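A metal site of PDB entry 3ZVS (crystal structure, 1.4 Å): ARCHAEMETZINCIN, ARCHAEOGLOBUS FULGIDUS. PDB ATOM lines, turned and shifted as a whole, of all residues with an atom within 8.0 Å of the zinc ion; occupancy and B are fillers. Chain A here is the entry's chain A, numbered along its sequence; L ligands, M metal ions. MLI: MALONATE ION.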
ATOM      1  N   PHE A  82      24.779   9.811  19.676  1.00  0.00           N
ATOM      2  CA  PHE A  82      23.975  10.403  20.733  1.00  0.00           C
ATOM      3  C   PHE A  82      23.130  11.546  20.213  1.00  0.00           C
ATOM      4  O   PHE A  82      22.126  11.932  20.821  1.00  0.00           O
ATOM      5  CB  PHE A  82      24.847  10.926  21.861  1.00  0.00           C
ATOM      6  CG  PHE A  82      25.601   9.859  22.602  1.00  0.00           C
ATOM      7  CD1 PHE A  82      24.937   8.934  23.403  1.00  0.00           C
ATOM      8  CD2 PHE A  82      27.004   9.809  22.575  1.00  0.00           C
ATOM      9  CE1 PHE A  82      25.617   7.970  24.121  1.00  0.00           C
ATOM     10  CE2 PHE A  82      27.676   8.830  23.264  1.00  0.00           C
ATOM     11  CZ  PHE A  82      26.983   7.895  24.048  1.00  0.00           C
ATOM     12  N   GLY A  83      23.519  12.123  19.085  1.00  0.00           N
ATOM     13  CA  GLY A  83      22.856  13.290  18.565  1.00  0.00           C
ATOM     14  C   GLY A  83      23.478  13.708  17.245  1.00  0.00           C
ATOM     15  O   GLY A  83      24.459  13.113  16.771  1.00  0.00           O
ATOM     16  N   GLU A  84      22.900  14.752  16.678  1.00  0.00           N
ATOM     17  CA  GLU A  84      23.409  15.403  15.479  1.00  0.00           C
ATOM     18  C   GLU A  84      22.969  16.862  15.542  1.00  0.00           C
ATOM     19  O   GLU A  84      21.862  17.179  16.009  1.00  0.00           O
ATOM     20  CB  GLU A  84      22.919  14.746  14.170  1.00  0.00           C
ATOM     21  CG  GLU A  84      23.690  15.317  12.933  1.00  0.00           C
ATOM     22  CD  GLU A  84      23.356  14.695  11.603  1.00  0.00           C
ATOM     23  OE1 GLU A  84      22.576  13.759  11.569  1.00  0.00           O
ATOM     24  OE2 GLU A  84      23.915  15.149  10.575  1.00  0.00           O
ATOM     25  N   ALA A  85      23.844  17.763  15.113  1.00  0.00           N
ATOM     26  CA  ALA A  85      23.586  19.172  15.169  1.00  0.00           C
ATOM     27  C   ALA A  85      24.031  19.885  13.910  1.00  0.00           C
ATOM     28  O   ALA A  85      24.982  19.450  13.237  1.00  0.00           O
ATOM     29  CB  ALA A  85      24.292  19.786  16.401  1.00  0.00           C
ATOM     30  N   GLU A 114      24.449  15.649  27.570  1.00  0.00           N
ATOM     31  CA  GLU A 114      24.370  15.412  26.144  1.00  0.00           C
ATOM     32  C   GLU A 114      23.493  16.444  25.442  1.00  0.00           C
ATOM     33  O   GLU A 114      23.761  16.826  24.282  1.00  0.00           O
ATOM     34  CB  GLU A 114      23.924  13.971  25.894  1.00  0.00           C
ATOM     35  CG  GLU A 114      24.969  12.960  26.405  1.00  0.00           C
ATOM     36  CD  GLU A 114      26.279  13.113  25.729  1.00  0.00           C
ATOM     37  OE1 GLU A 114      26.407  12.536  24.634  1.00  0.00           O
ATOM     38  OE2 GLU A 114      27.174  13.832  26.202  1.00  0.00           O
ATOM     39  N   HIS A 117      25.776  19.467  25.164  1.00  0.00           N
ATOM     40  CA  HIS A 117      26.728  19.181  24.081  1.00  0.00           C
ATOM     41  C   HIS A 117      26.133  19.534  22.705  1.00  0.00           C
ATOM     42  O   HIS A 117      26.723  20.205  21.872  1.00  0.00           O
ATOM     43  CB  HIS A 117      27.107  17.709  24.152  1.00  0.00           C
ATOM     44  CG  HIS A 117      28.092  17.288  23.116  1.00  0.00           C
ATOM     45  ND1 HIS A 117      29.455  17.258  23.351  1.00  0.00           N
ATOM     46  CD2 HIS A 117      27.929  16.907  21.813  1.00  0.00           C
ATOM     47  CE1 HIS A 117      30.079  16.841  22.252  1.00  0.00           C
ATOM     48  NE2 HIS A 117      29.172  16.619  21.308  1.00  0.00           N
ATOM     49  N   GLU A 118      24.926  19.035  22.454  1.00  0.00           N
ATOM     50  CA  GLU A 118      24.284  19.284  21.167  1.00  0.00           C
ATOM     51  C   GLU A 118      24.032  20.786  20.947  1.00  0.00           C
ATOM     52  O   GLU A 118      24.239  21.322  19.880  1.00  0.00           O
ATOM     53  CB  GLU A 118      22.960  18.505  21.059  1.00  0.00           C
ATOM     54  CG  GLU A 118      23.150  17.001  20.971  1.00  0.00           C
ATOM     55  CD  GLU A 118      24.134  16.579  19.915  1.00  0.00           C
ATOM     56  OE1 GLU A 118      24.109  17.146  18.788  1.00  0.00           O
ATOM     57  OE2 GLU A 118      24.969  15.691  20.169  1.00  0.00           O
ATOM     58  N   GLY A 120      25.612  23.236  22.293  1.00  0.00           N
ATOM     59  CA  GLY A 120      26.892  23.870  22.060  1.00  0.00           C
ATOM     60  C   GLY A 120      27.289  23.817  20.599  1.00  0.00           C
ATOM     61  O   GLY A 120      27.821  24.800  20.091  1.00  0.00           O
ATOM     62  N   HIS A 121      27.078  22.688  19.937  1.00  0.00           N
ATOM     63  CA  HIS A 121      27.321  22.632  18.494  1.00  0.00           C
ATOM     64  C   HIS A 121      26.471  23.626  17.712  1.00  0.00           C
ATOM     65  O   HIS A 121      26.968  24.276  16.795  1.00  0.00           O
ATOM     66  CB  HIS A 121      27.020  21.261  17.920  1.00  0.00           C
ATOM     67  CG  HIS A 121      28.031  20.177  18.217  1.00  0.00           C
ATOM     68  ND1 HIS A 121      29.389  20.315  18.031  1.00  0.00           N
ATOM     69  CD2 HIS A 121      27.832  18.891  18.587  1.00  0.00           C
ATOM     70  CE1 HIS A 121      29.983  19.146  18.284  1.00  0.00           C
ATOM     71  NE2 HIS A 121      29.053  18.278  18.644  1.00  0.00           N
ATOM     72  N   LEU A 125      30.203  25.627  18.468  1.00  0.00           N
ATOM     73  CA  LEU A 125      31.331  24.929  19.087  1.00  0.00           C
ATOM     74  C   LEU A 125      31.589  23.566  18.465  1.00  0.00           C
ATOM     75  O   LEU A 125      30.707  22.712  18.371  1.00  0.00           O
ATOM     76  CB  LEU A 125      31.124  24.738  20.593  1.00  0.00           C
ATOM     77  CG  LEU A 125      30.942  26.026  21.386  1.00  0.00           C
ATOM     78  CD1 LEU A 125      30.595  25.728  22.826  1.00  0.00           C
ATOM     79  CD2 LEU A 125      32.224  26.838  21.353  1.00  0.00           C
ATOM     80  N   LYS A 126      32.822  23.362  18.025  1.00  0.00           N
ATOM     81  CA  LYS A 126      33.297  22.053  17.600  1.00  0.00           C
ATOM     82  C   LYS A 126      33.724  21.202  18.795  1.00  0.00           C
ATOM     83  O   LYS A 126      33.750  21.660  19.939  1.00  0.00           O
ATOM     84  CB  LYS A 126      34.489  22.220  16.648  1.00  0.00           C
ATOM     85  CG  LYS A 126      34.125  22.983  15.396  1.00  0.00           C
ATOM     86  CD  LYS A 126      35.297  23.069  14.399  1.00  0.00           C
ATOM     87  CE  LYS A 126      35.108  24.265  13.463  1.00  0.00           C
ATOM     88  NZ  LYS A 126      35.117  25.597  14.183  1.00  0.00           N
ATOM     89  N   HIS A 127      33.994  19.924  18.559  1.00  0.00           N
ATOM     90  CA  HIS A 127      34.516  19.117  19.646  1.00  0.00           C
ATOM     91  C   HIS A 127      35.744  19.734  20.259  1.00  0.00           C
ATOM     92  O   HIS A 127      36.588  20.290  19.571  1.00  0.00           O
ATOM     93  CB  HIS A 127      34.773  17.689  19.189  1.00  0.00           C
ATOM     94  CG  HIS A 127      33.512  16.954  18.945  1.00  0.00           C
ATOM     95  ND1 HIS A 127      33.351  16.004  17.968  1.00  0.00           N
ATOM     96  CD2 HIS A 127      32.302  17.079  19.539  1.00  0.00           C
ATOM     97  CE1 HIS A 127      32.102  15.567  17.977  1.00  0.00           C
ATOM     98  NE2 HIS A 127      31.449  16.189  18.934  1.00  0.00           N
ATOM     99  N   CYS A 128      35.812  19.596  21.578  1.00  0.00           N
ATOM    100  CA  CYS A 128      36.847  20.206  22.402  1.00  0.00           C
ATOM    101  C   CYS A 128      37.629  19.104  23.103  1.00  0.00           C
ATOM    102  O   CYS A 128      37.064  18.133  23.622  1.00  0.00           O
ATOM    103  CB  CYS A 128      36.117  21.039  23.451  1.00  0.00           C
ATOM    104  SG  CYS A 128      37.277  21.961  24.561  1.00  0.00           S
ATOM    105  N   VAL A 133      32.290  19.756  28.454  1.00  0.00           N
ATOM    106  CA  VAL A 133      31.104  19.053  27.934  1.00  0.00           C
ATOM    107  C   VAL A 133      31.156  18.883  26.417  1.00  0.00           C
ATOM    108  O   VAL A 133      30.484  17.999  25.893  1.00  0.00           O
ATOM    109  CB  VAL A 133      29.853  19.847  28.369  1.00  0.00           C
ATOM    110  CG1 VAL A 133      29.750  21.194  27.660  1.00  0.00           C
ATOM    111  CG2 VAL A 133      28.591  19.021  28.191  1.00  0.00           C
ATOM    112  N   MET A 134      31.927  19.719  25.716  1.00  0.00           N
ATOM    113  CA  MET A 134      32.095  19.599  24.280  1.00  0.00           C
ATOM    114  C   MET A 134      33.054  18.517  23.818  1.00  0.00           C
ATOM    115  O   MET A 134      33.218  18.322  22.608  1.00  0.00           O
ATOM    116  CB  MET A 134      32.460  20.963  23.617  1.00  0.00           C
ATOM    117  CG  MET A 134      31.322  22.024  23.659  1.00  0.00           C
ATOM    118  SD  MET A 134      29.698  21.417  23.104  1.00  0.00           S
ATOM    119  CE  MET A 134      30.093  20.799  21.437  1.00  0.00           C
ATOM    120  N   ARG A 135      33.653  17.767  24.737  1.00  0.00           N
ATOM    121  CA  ARG A 135      34.397  16.570  24.312  1.00  0.00           C
ATOM    122  C   ARG A 135      33.476  15.633  23.582  1.00  0.00           C
ATOM    123  O   ARG A 135      32.320  15.400  24.005  1.00  0.00           O
ATOM    124  CB  ARG A 135      34.891  15.782  25.519  1.00  0.00           C
ATOM    125  CG  ARG A 135      36.090  16.311  26.240  1.00  0.00           C
ATOM    126  CD  ARG A 135      36.563  15.180  27.198  1.00  0.00           C
ATOM    127  NE  ARG A 135      37.420  15.676  28.279  1.00  0.00           N
ATOM    128  CZ  ARG A 135      37.548  15.089  29.452  1.00  0.00           C
ATOM    129  NH1 ARG A 135      36.861  13.988  29.764  1.00  0.00           N
ATOM    130  NH2 ARG A 135      38.390  15.623  30.331  1.00  0.00           N
ATOM    131  N   PHE A 136      33.949  15.055  22.481  1.00  0.00           N
ATOM    132  CA  PHE A 136      33.285  13.889  21.913  1.00  0.00           C
ATOM    133  C   PHE A 136      33.287  12.733  22.897  1.00  0.00           C
ATOM    134  O   PHE A 136      34.318  12.478  23.563  1.00  0.00           O
ATOM    135  CB  PHE A 136      33.993  13.467  20.640  1.00  0.00           C
ATOM    136  CG  PHE A 136      33.479  12.178  20.052  1.00  0.00           C
ATOM    137  CD1 PHE A 136      32.344  12.156  19.257  1.00  0.00           C
ATOM    138  CD2 PHE A 136      34.108  10.970  20.346  1.00  0.00           C
ATOM    139  CE1 PHE A 136      31.865  10.975  18.741  1.00  0.00           C
ATOM    140  CE2 PHE A 136      33.631   9.778  19.810  1.00  0.00           C
ATOM    141  CZ  PHE A 136      32.496   9.797  19.023  1.00  0.00           C
ATOM    142  N   SER A 137      32.167  12.026  23.006  1.00  0.00           N
ATOM    143  CA  SER A 137      32.077  10.825  23.826  1.00  0.00           C
ATOM    144  C   SER A 137      31.813   9.619  22.980  1.00  0.00           C
ATOM    145  O   SER A 137      30.807   9.566  22.251  1.00  0.00           O
ATOM    146  CB  SER A 137      30.965  10.937  24.877  1.00  0.00           C
ATOM    147  OG  SER A 137      31.179  12.034  25.742  1.00  0.00           O
ATOM    148  N   LYS A 146      33.255  13.189  31.356  1.00  0.00           N
ATOM    149  CA  LYS A 146      33.314  14.602  31.016  1.00  0.00           C
ATOM    150  C   LYS A 146      32.357  15.421  31.886  1.00  0.00           C
ATOM    151  O   LYS A 146      31.383  14.913  32.417  1.00  0.00           O
ATOM    152  CB  LYS A 146      33.024  14.823  29.543  1.00  0.00           C
ATOM    153  CG  LYS A 146      31.534  14.816  29.125  1.00  0.00           C
ATOM    154  CD  LYS A 146      31.448  14.927  27.578  1.00  0.00           C
ATOM    155  CE  LYS A 146      30.026  14.916  27.067  1.00  0.00           C
ATOM    156  NZ  LYS A 146      30.021  14.594  25.573  1.00  0.00           N
HETATM  157  C1  MLI L   1      27.473  12.998  18.013  1.00  0.00           C
HETATM  158  C2  MLI L   1      28.419  13.970  18.639  1.00  0.00           C
HETATM  159  C3  MLI L   1      27.766  11.572  18.256  1.00  0.00           C
HETATM  160  O6  MLI L   1      29.411  13.556  19.287  1.00  0.00           O
HETATM  161  O7  MLI L   1      28.111  15.158  18.531  1.00  0.00           O
HETATM  162  O8  MLI L   1      28.435  10.930  17.440  1.00  0.00           O
HETATM  163  O9  MLI L   1      27.375  10.981  19.305  1.00  0.00           O
HETATM  164 ZN    ZN M   1      29.488  16.358  19.282  1.00  0.00          ZN
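A ring nitrogen (ND1) of His 121 is in hydrogen-bond range of the backbone carbonyl oxygen of Leu 125, 2.8 Å away.
A ring nitrogen (ND1) of His 117 is in hydrogen-bond range of the backbone carbonyl oxygen (O) of Val 133 (2.8 Å).
A ring nitrogen (ND1) of His 117 lies close to the backbone carbonyl oxygen (O) of Arg 135 (3.5 Å).
O7 of the ligand binds the zinc ion (2.0 Å).
NE2 of His 127 binds the zinc ion.
The zinc ion is bound by NE2 of His 117, 2.1 Å away.
The zinc ion is bound by NE2 of His 121, 2.1 Å away.
The zinc ion has four donor atoms within binding distance.
Slightly farther from the zinc ion lies O6 of the ligand (2.8 Å).
Of the 19 residues printed, 3 come within 4 Å of the zinc ion.
The nearest printed residue that does not touch the zinc ion is Glu 118 (4.7 Å).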
